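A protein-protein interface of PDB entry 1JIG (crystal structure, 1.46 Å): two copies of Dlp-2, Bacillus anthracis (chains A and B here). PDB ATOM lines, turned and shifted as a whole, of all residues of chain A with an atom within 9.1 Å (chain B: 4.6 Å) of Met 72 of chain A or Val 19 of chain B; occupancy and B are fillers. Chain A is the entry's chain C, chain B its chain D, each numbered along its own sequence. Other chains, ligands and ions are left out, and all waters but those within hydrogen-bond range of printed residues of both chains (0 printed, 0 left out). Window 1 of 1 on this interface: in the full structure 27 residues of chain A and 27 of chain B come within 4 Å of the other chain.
O of Tyr 75 of chain B lies within hydrogen-bond range of OG of Ser 79 of chain B, 3.1 Å away. The side-chain hydroxyl (OH) of Tyr 75 of chain B lies close to the side-chain amide nitrogen (ND2) of Asn 18 of chain B (3.5 Å). O of Tyr 75 of chain A sits at hydrogen-bond distance from OG of Ser 79 of chain A, at 3.1 Å. The side-chain amide nitrogen of Asn 18 of chain A sits close to the side-chain hydroxyl of Tyr 75 of chain A (3.5 Å). The side-chain hydroxyl of Tyr 75 of chain A lies within hydrogen-bond range of the backbone carbonyl oxygen of Leu 69 of chain A, at 2.8 Å. The backbone carbonyl oxygen (O) of Tyr 75 of chain A lies within hydrogen-bond range of the side-chain hydroxyl (OG1) of Thr 78 of chain A (3.2 Å).
Asn 18 of chain A touches Met 72 of chain B, and with the chains exchanged Met 72 of chain A touches Asn 18 of chain B. Val 19 of chain A touches Met 72 of chain B, and with the chains exchanged Met 72 of chain A touches Val 19 of chain B. Val 22 of chain A touches Tyr 75 of chain B, and with the chains exchanged Tyr 75 of chain A touches Val 22 of chain B. Met 72 of chain A touches Leu 76 of chain B, and with the chains exchanged Leu 76 of chain A touches Met 72 of chain B. Positions printed for both chains: 15, 18, 19, 21, 22, 72, 75, 76, 79 and 83. Of the 22 pairs that touch across the chains among the printed residues, 17 have their exchanged pair printed and touching as well.
Among the printed residues, pairs that only touch across the chains: Asn 18 of chain A with Val 22 of chain B, Asn 18 of chain A with Met 72 of chain B, Val 19 of chain A with Met 72 of chain B, Tyr 21 of chain A with Tyr 21 of chain B, Val 22 of chain A with Asn 18 of chain B, Val 22 of chain A with Tyr 75 of chain B, Ala 70 of chain A with Val 22 of chain B, Thr 71 of chain A with Val 22 of chain B, Thr 71 of chain A with Glu 83 of chain B, Met 72 of chain A with Asn 18 of chain B, Met 72 of chain A with Val 19 of chain B, Met 72 of chain A with Met 72 of chain B, Met 72 of chain A with Tyr 75 of chain B, Met 72 of chain A with Leu 76 of chain B, Lys 73 of chain A with Leu 76 of chain B, Tyr 75 of chain A with Val 22 of chain B, Tyr 75 of chain A with Met 72 of chain B, Leu 76 of chain A with Met 72 of chain B and Leu 76 of chain A with Leu 76 of chain B.
The backbone NH (N) of Met 72 of chain B lies close to the side-chain carboxylate (OE1) of Glu 83 of chain A (3.1 Å). The backbone NH (N) of Lys 73 of chain A sits at hydrogen-bond distance from the side-chain carboxylate (OE1) of Glu 83 of chain B, 3.1 Å away. N of Met 72 of chain A lies close to OE1 of Glu 83 of chain B, 3.1 Å away.
Hydrophobic or aromatic side chains of chain B that line the printed part of chain A: Tyr 21, Val 22, Met 72, Tyr 75 and Leu 76. Printed residues of chain A that touch a printed residue of chain B: Asn 18, Val 19, Tyr 21, Val 22, Ala 70, Thr 71, Met 72, Lys 73, Tyr 75, Leu 76 and Glu 83. Among the printed residues, 22 pairs touch across the chains. Among the printed residues, no Asp or Glu carboxylate lies within 4 Å of a Lys or Arg side-chain nitrogen of the other chain.
Of chain A, only Met 72 comes within 4 Å of Val 19 of chain B. Of the printed residues of chain A, Tyr 21 of chain B touches Tyr 21. Of the printed residues of chain B, Glu 83 of chain A touches Met 72. Of the printed residues of chain B, Thr 71 of chain A touches Val 22 (3.9 Å) and Glu 83 (3.4 Å). Thr 78 of chain A touches none of the printed residues of chain B.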
ATOM      1  N   ALA A  15      -9.209  -3.695 -11.339  1.00  0.00           N
ATOM      2  CA  ALA A  15     -10.098  -2.767 -10.658  1.00  0.00           C
ATOM      3  C   ALA A  15     -10.779  -1.837 -11.668  1.00  0.00           C
ATOM      4  O   ALA A  15     -12.004  -1.688 -11.655  1.00  0.00           O
ATOM      5  CB  ALA A  15      -9.321  -1.953  -9.646  1.00  0.00           C
ATOM      6  N   ASN A  18     -13.498  -3.471 -13.759  1.00  0.00           N
ATOM      7  CA  ASN A  18     -14.673  -3.870 -13.012  1.00  0.00           C
ATOM      8  C   ASN A  18     -15.541  -2.621 -12.885  1.00  0.00           C
ATOM      9  O   ASN A  18     -16.748  -2.679 -13.100  1.00  0.00           O
ATOM     10  CB  ASN A  18     -14.275  -4.412 -11.639  1.00  0.00           C
ATOM     11  CG  ASN A  18     -14.098  -5.915 -11.652  1.00  0.00           C
ATOM     12  OD1 ASN A  18     -15.060  -6.658 -11.463  1.00  0.00           O
ATOM     13  ND2 ASN A  18     -12.884  -6.370 -11.914  1.00  0.00           N
ATOM     14  N   VAL A  19     -14.917  -1.495 -12.549  1.00  0.00           N
ATOM     15  CA  VAL A  19     -15.638  -0.234 -12.426  1.00  0.00           C
ATOM     16  C   VAL A  19     -16.245   0.168 -13.777  1.00  0.00           C
ATOM     17  O   VAL A  19     -17.349   0.709 -13.828  1.00  0.00           O
ATOM     18  CB  VAL A  19     -14.708   0.892 -11.935  1.00  0.00           C
ATOM     19  CG1 VAL A  19     -15.474   2.216 -11.871  1.00  0.00           C
ATOM     20  CG2 VAL A  19     -14.148   0.530 -10.569  1.00  0.00           C
ATOM     21  N   TYR A  21     -17.059  -1.958 -16.160  1.00  0.00           N
ATOM     22  CA  TYR A  21     -18.113  -2.906 -16.481  1.00  0.00           C
ATOM     23  C   TYR A  21     -19.432  -2.333 -15.968  1.00  0.00           C
ATOM     24  O   TYR A  21     -20.425  -2.321 -16.685  1.00  0.00           O
ATOM     25  CB  TYR A  21     -17.811  -4.255 -15.831  1.00  0.00           C
ATOM     26  CG  TYR A  21     -18.879  -5.311 -16.005  1.00  0.00           C
ATOM     27  CD1 TYR A  21     -19.840  -5.522 -15.016  1.00  0.00           C
ATOM     28  CD2 TYR A  21     -18.902  -6.137 -17.134  1.00  0.00           C
ATOM     29  CE1 TYR A  21     -20.798  -6.533 -15.136  1.00  0.00           C
ATOM     30  CE2 TYR A  21     -19.861  -7.155 -17.264  1.00  0.00           C
ATOM     31  CZ  TYR A  21     -20.805  -7.346 -16.254  1.00  0.00           C
ATOM     32  OH  TYR A  21     -21.745  -8.357 -16.345  1.00  0.00           O
ATOM     33  N   VAL A  22     -19.432  -1.847 -14.729  1.00  0.00           N
ATOM     34  CA  VAL A  22     -20.627  -1.247 -14.126  1.00  0.00           C
ATOM     35  C   VAL A  22     -21.013   0.074 -14.821  1.00  0.00           C
ATOM     36  O   VAL A  22     -22.176   0.306 -15.143  1.00  0.00           O
ATOM     37  CB  VAL A  22     -20.402  -0.976 -12.604  1.00  0.00           C
ATOM     38  CG1 VAL A  22     -21.551  -0.151 -12.037  1.00  0.00           C
ATOM     39  CG2 VAL A  22     -20.268  -2.305 -11.849  1.00  0.00           C
ATOM     40  N   LEU A  69      -7.140  -8.709  -7.280  1.00  0.00           N
ATOM     41  CA  LEU A  69      -8.117  -8.039  -6.424  1.00  0.00           C
ATOM     42  C   LEU A  69      -9.463  -8.695  -6.752  1.00  0.00           C
ATOM     43  O   LEU A  69      -9.805  -8.868  -7.931  1.00  0.00           O
ATOM     44  CB  LEU A  69      -8.170  -6.535  -6.719  1.00  0.00           C
ATOM     45  CG  LEU A  69      -6.913  -5.717  -6.398  1.00  0.00           C
ATOM     46  CD1 LEU A  69      -7.149  -4.242  -6.728  1.00  0.00           C
ATOM     47  CD2 LEU A  69      -6.564  -5.875  -4.920  1.00  0.00           C
ATOM     48  N   ALA A  70     -10.223  -9.069  -5.724  1.00  0.00           N
ATOM     49  CA  ALA A  70     -11.502  -9.729  -5.966  1.00  0.00           C
ATOM     50  C   ALA A  70     -12.675  -9.305  -5.080  1.00  0.00           C
ATOM     51  O   ALA A  70     -13.508 -10.130  -4.701  1.00  0.00           O
ATOM     52  CB  ALA A  70     -11.318 -11.238  -5.910  1.00  0.00           C
ATOM     53  N   THR A  71     -12.730  -8.020  -4.744  1.00  0.00           N
ATOM     54  CA  THR A  71     -13.853  -7.481  -3.982  1.00  0.00           C
ATOM     55  C   THR A  71     -14.164  -6.110  -4.541  1.00  0.00           C
ATOM     56  O   THR A  71     -13.288  -5.401  -5.050  1.00  0.00           O
ATOM     57  CB  THR A  71     -13.592  -7.339  -2.451  1.00  0.00           C
ATOM     58  OG1 THR A  71     -12.576  -6.355  -2.213  1.00  0.00           O
ATOM     59  CG2 THR A  71     -13.209  -8.686  -1.846  1.00  0.00           C
ATOM     60  N   MET A  72     -15.432  -5.754  -4.461  1.00  0.00           N
ATOM     61  CA  MET A  72     -15.905  -4.469  -4.940  1.00  0.00           C
ATOM     62  C   MET A  72     -15.275  -3.352  -4.103  1.00  0.00           C
ATOM     63  O   MET A  72     -14.913  -2.297  -4.613  1.00  0.00           O
ATOM     64  CB  MET A  72     -17.420  -4.443  -4.816  1.00  0.00           C
ATOM     65  CG  MET A  72     -18.109  -3.917  -6.017  1.00  0.00           C
ATOM     66  SD  MET A  72     -19.894  -4.042  -5.907  1.00  0.00           S
ATOM     67  CE  MET A  72     -20.225  -4.927  -7.399  1.00  0.00           C
ATOM     68  N   LYS A  73     -15.141  -3.601  -2.807  1.00  0.00           N
ATOM     69  CA  LYS A  73     -14.547  -2.628  -1.905  1.00  0.00           C
ATOM     70  C   LYS A  73     -13.136  -2.283  -2.362  1.00  0.00           C
ATOM     71  O   LYS A  73     -12.717  -1.127  -2.289  1.00  0.00           O
ATOM     72  CB  LYS A  73     -14.491  -3.186  -0.488  1.00  0.00           C
ATOM     73  CG  LYS A  73     -14.105  -2.146   0.531  1.00  0.00           C
ATOM     74  CD  LYS A  73     -14.143  -2.680   1.945  1.00  0.00           C
ATOM     75  CE  LYS A  73     -14.349  -1.525   2.911  1.00  0.00           C
ATOM     76  NZ  LYS A  73     -13.462  -0.389   2.550  1.00  0.00           N
ATOM     77  N   GLU A  74     -12.405  -3.290  -2.833  1.00  0.00           N
ATOM     78  CA  GLU A  74     -11.039  -3.087  -3.300  1.00  0.00           C
ATOM     79  C   GLU A  74     -10.971  -2.411  -4.662  1.00  0.00           C
ATOM     80  O   GLU A  74     -10.065  -1.618  -4.915  1.00  0.00           O
ATOM     81  CB  GLU A  74     -10.283  -4.418  -3.328  1.00  0.00           C
ATOM     82  CG  GLU A  74      -9.865  -4.891  -1.944  1.00  0.00           C
ATOM     83  CD  GLU A  74      -8.999  -3.863  -1.226  1.00  0.00           C
ATOM     84  OE1 GLU A  74      -8.735  -4.035  -0.009  1.00  0.00           O
ATOM     85  OE2 GLU A  74      -8.579  -2.882  -1.887  1.00  0.00           O
ATOM     86  N   TYR A  75     -11.920  -2.717  -5.539  1.00  0.00           N
ATOM     87  CA  TYR A  75     -11.945  -2.089  -6.860  1.00  0.00           C
ATOM     88  C   TYR A  75     -12.175  -0.585  -6.706  1.00  0.00           C
ATOM     89  O   TYR A  75     -11.524   0.233  -7.357  1.00  0.00           O
ATOM     90  CB  TYR A  75     -13.065  -2.690  -7.725  1.00  0.00           C
ATOM     91  CG  TYR A  75     -12.876  -4.155  -8.044  1.00  0.00           C
ATOM     92  CD1 TYR A  75     -11.599  -4.698  -8.168  1.00  0.00           C
ATOM     93  CD2 TYR A  75     -13.968  -4.996  -8.247  1.00  0.00           C
ATOM     94  CE1 TYR A  75     -11.412  -6.040  -8.490  1.00  0.00           C
ATOM     95  CE2 TYR A  75     -13.787  -6.343  -8.567  1.00  0.00           C
ATOM     96  CZ  TYR A  75     -12.507  -6.852  -8.687  1.00  0.00           C
ATOM     97  OH  TYR A  75     -12.315  -8.171  -9.006  1.00  0.00           O
ATOM     98  N   LEU A  76     -13.099  -0.226  -5.825  1.00  0.00           N
ATOM     99  CA  LEU A  76     -13.420   1.175  -5.580  1.00  0.00           C
ATOM    100  C   LEU A  76     -12.259   1.921  -4.944  1.00  0.00           C
ATOM    101  O   LEU A  76     -12.059   3.103  -5.197  1.00  0.00           O
ATOM    102  CB  LEU A  76     -14.639   1.279  -4.669  1.00  0.00           C
ATOM    103  CG  LEU A  76     -15.999   1.087  -5.329  1.00  0.00           C
ATOM    104  CD1 LEU A  76     -17.059   0.871  -4.258  1.00  0.00           C
ATOM    105  CD2 LEU A  76     -16.318   2.304  -6.188  1.00  0.00           C
ATOM    106  N   ALA A  77     -11.494   1.228  -4.113  1.00  0.00           N
ATOM    107  CA  ALA A  77     -10.376   1.855  -3.437  1.00  0.00           C
ATOM    108  C   ALA A  77      -9.154   1.909  -4.326  1.00  0.00           C
ATOM    109  O   ALA A  77      -8.191   2.613  -4.018  1.00  0.00           O
ATOM    110  CB  ALA A  77     -10.052   1.095  -2.161  1.00  0.00           C
ATOM    111  N   THR A  78      -9.194   1.176  -5.438  1.00  0.00           N
ATOM    112  CA  THR A  78      -8.049   1.111  -6.340  1.00  0.00           C
ATOM    113  C   THR A  78      -8.204   1.738  -7.729  1.00  0.00           C
ATOM    114  O   THR A  78      -7.254   2.315  -8.260  1.00  0.00           O
ATOM    115  CB  THR A  78      -7.587  -0.367  -6.516  1.00  0.00           C
ATOM    116  OG1 THR A  78      -8.649  -1.148  -7.076  1.00  0.00           O
ATOM    117  CG2 THR A  78      -7.225  -0.974  -5.176  1.00  0.00           C
ATOM    118  N   SER A  79      -9.387   1.632  -8.320  1.00  0.00           N
ATOM    119  CA  SER A  79      -9.592   2.165  -9.661  1.00  0.00           C
ATOM    120  C   SER A  79      -9.447   3.668  -9.745  1.00  0.00           C
ATOM    121  O   SER A  79      -9.693   4.396  -8.780  1.00  0.00           O
ATOM    122  CB  SER A  79     -10.964   1.754 -10.210  1.00  0.00           C
ATOM    123  OG  SER A  79     -12.017   2.380  -9.503  1.00  0.00           O
ATOM    124  N   GLU A  83     -17.147   6.592 -11.256  1.00  0.00           N
ATOM    125  CA  GLU A  83     -18.357   5.861 -11.607  1.00  0.00           C
ATOM    126  C   GLU A  83     -19.363   6.784 -12.288  1.00  0.00           C
ATOM    127  O   GLU A  83     -19.291   8.013 -12.152  1.00  0.00           O
ATOM    128  CB  GLU A  83     -18.984   5.223 -10.362  1.00  0.00           C
ATOM    129  CG  GLU A  83     -18.147   4.086  -9.775  1.00  0.00           C
ATOM    130  CD  GLU A  83     -18.954   3.147  -8.903  1.00  0.00           C
ATOM    131  OE1 GLU A  83     -19.254   3.497  -7.744  1.00  0.00           O
ATOM    132  OE2 GLU A  83     -19.299   2.055  -9.387  1.00  0.00           O
ATOM    133  N   ALA B  15     -28.256  -5.140  -7.318  1.00  0.00           N
ATOM    134  CA  ALA B  15     -27.115  -4.999  -6.428  1.00  0.00           C
ATOM    135  C   ALA B  15     -26.539  -6.374  -6.073  1.00  0.00           C
ATOM    136  O   ALA B  15     -25.335  -6.599  -6.201  1.00  0.00           O
ATOM    137  CB  ALA B  15     -27.532  -4.270  -5.167  1.00  0.00           C
ATOM    138  N   ASN B  16     -27.391  -7.298  -5.632  1.00  0.00           N
ATOM    139  CA  ASN B  16     -26.931  -8.640  -5.267  1.00  0.00           C
ATOM    140  C   ASN B  16     -26.179  -9.336  -6.392  1.00  0.00           C
ATOM    141  O   ASN B  16     -25.122  -9.915  -6.172  1.00  0.00           O
ATOM    142  CB  ASN B  16     -28.092  -9.555  -4.866  1.00  0.00           C
ATOM    143  CG  ASN B  16     -28.744  -9.160  -3.565  1.00  0.00           C
ATOM    144  OD1 ASN B  16     -28.143  -8.503  -2.714  1.00  0.00           O
ATOM    145  ND2 ASN B  16     -29.995  -9.584  -3.392  1.00  0.00           N
ATOM    146  N   TRP B  17     -26.725  -9.290  -7.602  1.00  0.00           N
ATOM    147  CA  TRP B  17     -26.069  -9.975  -8.703  1.00  0.00           C
ATOM    148  C   TRP B  17     -24.781  -9.339  -9.189  1.00  0.00           C
ATOM    149  O   TRP B  17     -23.950 -10.001  -9.825  1.00  0.00           O
ATOM    150  CB  TRP B  17     -27.064 -10.230  -9.840  1.00  0.00           C
ATOM    151  CG  TRP B  17     -27.815 -11.497  -9.563  1.00  0.00           C
ATOM    152  CD1 TRP B  17     -27.269 -12.738  -9.354  1.00  0.00           C
ATOM    153  CD2 TRP B  17     -29.226 -11.647  -9.371  1.00  0.00           C
ATOM    154  NE1 TRP B  17     -28.252 -13.642  -9.038  1.00  0.00           N
ATOM    155  CE2 TRP B  17     -29.462 -13.002  -9.043  1.00  0.00           C
ATOM    156  CE3 TRP B  17     -30.315 -10.771  -9.447  1.00  0.00           C
ATOM    157  CZ2 TRP B  17     -30.743 -13.502  -8.787  1.00  0.00           C
ATOM    158  CZ3 TRP B  17     -31.596 -11.273  -9.193  1.00  0.00           C
ATOM    159  CH2 TRP B  17     -31.793 -12.628  -8.867  1.00  0.00           C
ATOM    160  N   ASN B  18     -24.593  -8.067  -8.866  1.00  0.00           N
ATOM    161  CA  ASN B  18     -23.355  -7.406  -9.223  1.00  0.00           C
ATOM    162  C   ASN B  18     -22.311  -7.891  -8.223  1.00  0.00           C
ATOM    163  O   ASN B  18     -21.199  -8.246  -8.608  1.00  0.00           O
ATOM    164  CB  ASN B  18     -23.514  -5.886  -9.161  1.00  0.00           C
ATOM    165  CG  ASN B  18     -23.899  -5.303 -10.503  1.00  0.00           C
ATOM    166  OD1 ASN B  18     -23.032  -4.993 -11.323  1.00  0.00           O
ATOM    167  ND2 ASN B  18     -25.191  -5.191 -10.753  1.00  0.00           N
ATOM    168  N   VAL B  19     -22.681  -7.919  -6.944  1.00  0.00           N
ATOM    169  CA  VAL B  19     -21.773  -8.387  -5.902  1.00  0.00           C
ATOM    170  C   VAL B  19     -21.419  -9.862  -6.133  1.00  0.00           C
ATOM    171  O   VAL B  19     -20.288 -10.274  -5.898  1.00  0.00           O
ATOM    172  CB  VAL B  19     -22.399  -8.228  -4.503  1.00  0.00           C
ATOM    173  CG1 VAL B  19     -21.446  -8.776  -3.433  1.00  0.00           C
ATOM    174  CG2 VAL B  19     -22.706  -6.758  -4.247  1.00  0.00           C
ATOM    175  N   LEU B  20     -22.400 -10.644  -6.584  1.00  0.00           N
ATOM    176  CA  LEU B  20     -22.197 -12.067  -6.873  1.00  0.00           C
ATOM    177  C   LEU B  20     -21.322 -12.255  -8.101  1.00  0.00           C
ATOM    178  O   LEU B  20     -20.541 -13.200  -8.177  1.00  0.00           O
ATOM    179  CB  LEU B  20     -23.536 -12.774  -7.103  1.00  0.00           C
ATOM    180  CG  LEU B  20     -24.150 -13.429  -5.871  1.00  0.00           C
ATOM    181  CD1 LEU B  20     -23.242 -14.542  -5.376  1.00  0.00           C
ATOM    182  CD2 LEU B  20     -24.346 -12.397  -4.791  1.00  0.00           C
ATOM    183  N   TYR B  21     -21.458 -11.356  -9.071  1.00  0.00           N
ATOM    184  CA  TYR B  21     -20.651 -11.442 -10.274  1.00  0.00           C
ATOM    185  C   TYR B  21     -19.183 -11.383  -9.861  1.00  0.00           C
ATOM    186  O   TYR B  21     -18.382 -12.189 -10.312  1.00  0.00           O
ATOM    187  CB  TYR B  21     -21.001 -10.291 -11.216  1.00  0.00           C
ATOM    188  CG  TYR B  21     -20.157 -10.204 -12.471  1.00  0.00           C
ATOM    189  CD1 TYR B  21     -19.048  -9.357 -12.529  1.00  0.00           C
ATOM    190  CD2 TYR B  21     -20.488 -10.934 -13.618  1.00  0.00           C
ATOM    191  CE1 TYR B  21     -18.288  -9.230 -13.695  1.00  0.00           C
ATOM    192  CE2 TYR B  21     -19.730 -10.813 -14.792  1.00  0.00           C
ATOM    193  CZ  TYR B  21     -18.631  -9.954 -14.822  1.00  0.00           C
ATOM    194  OH  TYR B  21     -17.885  -9.801 -15.979  1.00  0.00           O
ATOM    195  N   VAL B  22     -18.844 -10.436  -8.989  1.00  0.00           N
ATOM    196  CA  VAL B  22     -17.470 -10.288  -8.496  1.00  0.00           C
ATOM    197  C   VAL B  22     -17.056 -11.478  -7.607  1.00  0.00           C
ATOM    198  O   VAL B  22     -15.967 -12.024  -7.751  1.00  0.00           O
ATOM    199  CB  VAL B  22     -17.319  -8.967  -7.686  1.00  0.00           C
ATOM    200  CG1 VAL B  22     -15.965  -8.925  -6.978  1.00  0.00           C
ATOM    201  CG2 VAL B  22     -17.471  -7.764  -8.622  1.00  0.00           C
ATOM    202  N   LYS B  23     -17.931 -11.871  -6.688  1.00  0.00           N
ATOM    203  CA  LYS B  23     -17.640 -12.984  -5.779  1.00  0.00           C
ATOM    204  C   LYS B  23     -17.401 -14.286  -6.543  1.00  0.00           C
ATOM    205  O   LYS B  23     -16.548 -15.091  -6.166  1.00  0.00           O
ATOM    206  CB  LYS B  23     -18.796 -13.179  -4.795  1.00  0.00           C
ATOM    207  CG  LYS B  23     -18.459 -14.029  -3.577  1.00  0.00           C
ATOM    208  CD  LYS B  23     -19.639 -14.074  -2.612  1.00  0.00           C
ATOM    209  CE  LYS B  23     -19.230 -14.631  -1.258  1.00  0.00           C
ATOM    210  NZ  LYS B  23     -20.372 -14.646  -0.302  1.00  0.00           N
ATOM    211  N   MET B  72     -21.063   1.013  -8.171  1.00  0.00           N
ATOM    212  CA  MET B  72     -20.524   0.022  -7.259  1.00  0.00           C
ATOM    213  C   MET B  72     -20.788   0.458  -5.813  1.00  0.00           C
ATOM    214  O   MET B  72     -21.082  -0.354  -4.941  1.00  0.00           O
ATOM    215  CB  MET B  72     -19.032  -0.098  -7.512  1.00  0.00           C
ATOM    216  CG  MET B  72     -18.556  -1.494  -7.594  1.00  0.00           C
ATOM    217  SD  MET B  72     -16.837  -1.608  -8.072  1.00  0.00           S
ATOM    218  CE  MET B  72     -16.977  -2.689  -9.456  1.00  0.00           C
ATOM    219  N   TYR B  75     -24.245  -0.608  -5.007  1.00  0.00           N
ATOM    220  CA  TYR B  75     -24.415  -2.056  -4.894  1.00  0.00           C
ATOM    221  C   TYR B  75     -23.943  -2.517  -3.516  1.00  0.00           C
ATOM    222  O   TYR B  75     -24.590  -3.331  -2.856  1.00  0.00           O
ATOM    223  CB  TYR B  75     -23.609  -2.788  -5.981  1.00  0.00           C
ATOM    224  CG  TYR B  75     -24.069  -2.498  -7.392  1.00  0.00           C
ATOM    225  CD1 TYR B  75     -25.407  -2.224  -7.660  1.00  0.00           C
ATOM    226  CD2 TYR B  75     -23.174  -2.514  -8.461  1.00  0.00           C
ATOM    227  CE1 TYR B  75     -25.847  -1.975  -8.953  1.00  0.00           C
ATOM    228  CE2 TYR B  75     -23.604  -2.266  -9.763  1.00  0.00           C
ATOM    229  CZ  TYR B  75     -24.941  -2.000 -10.000  1.00  0.00           C
ATOM    230  OH  TYR B  75     -25.371  -1.762 -11.279  1.00  0.00           O
ATOM    231  N   LEU B  76     -22.805  -1.986  -3.085  1.00  0.00           N
ATOM    232  CA  LEU B  76     -22.238  -2.336  -1.789  1.00  0.00           C
ATOM    233  C   LEU B  76     -23.115  -1.867  -0.641  1.00  0.00           C
ATOM    234  O   LEU B  76     -23.195  -2.522   0.393  1.00  0.00           O
ATOM    235  CB  LEU B  76     -20.849  -1.718  -1.644  1.00  0.00           C
ATOM    236  CG  LEU B  76     -19.706  -2.454  -2.338  1.00  0.00           C
ATOM    237  CD1 LEU B  76     -18.490  -1.544  -2.414  1.00  0.00           C
ATOM    238  CD2 LEU B  76     -19.390  -3.737  -1.572  1.00  0.00           C
ATOM    239  N   SER B  79     -26.660  -4.424  -1.453  1.00  0.00           N
ATOM    240  CA  SER B  79     -26.671  -5.883  -1.465  1.00  0.00           C
ATOM    241  C   SER B  79     -26.606  -6.507  -0.089  1.00  0.00           C
ATOM    242  O   SER B  79     -26.049  -5.941   0.851  1.00  0.00           O
ATOM    243  CB  SER B  79     -25.528  -6.436  -2.322  1.00  0.00           C
ATOM    244  OG  SER B  79     -24.273  -6.198  -1.718  1.00  0.00           O
ATOM    245  N   VAL B  81     -25.447  -9.629   0.126  1.00  0.00           N
ATOM    246  CA  VAL B  81     -24.451 -10.674  -0.045  1.00  0.00           C
ATOM    247  C   VAL B  81     -23.062 -10.197   0.374  1.00  0.00           C
ATOM    248  O   VAL B  81     -22.602  -9.127  -0.035  1.00  0.00           O
ATOM    249  CB  VAL B  81     -24.413 -11.158  -1.514  1.00  0.00           C
ATOM    250  CG1 VAL B  81     -25.737 -11.811  -1.883  1.00  0.00           C
ATOM    251  CG2 VAL B  81     -24.163  -9.982  -2.434  1.00  0.00           C
ATOM    252  N   GLU B  83     -19.066 -10.117   0.419  1.00  0.00           N
ATOM    253  CA  GLU B  83     -18.083 -10.340  -0.630  1.00  0.00           C
ATOM    254  C   GLU B  83     -17.125 -11.459  -0.236  1.00  0.00           C
ATOM    255  O   GLU B  83     -16.985 -11.788   0.948  1.00  0.00           O
ATOM    256  CB  GLU B  83     -17.302  -9.055  -0.922  1.00  0.00           C
ATOM    257  CG  GLU B  83     -18.148  -7.967  -1.573  1.00  0.00           C
ATOM    258  CD  GLU B  83     -17.313  -6.944  -2.311  1.00  0.00           C
ATOM    259  OE1 GLU B  83     -16.730  -6.047  -1.664  1.00  0.00           O
ATOM    260  OE2 GLU B  83     -17.233  -7.050  -3.547  1.00  0.00           O
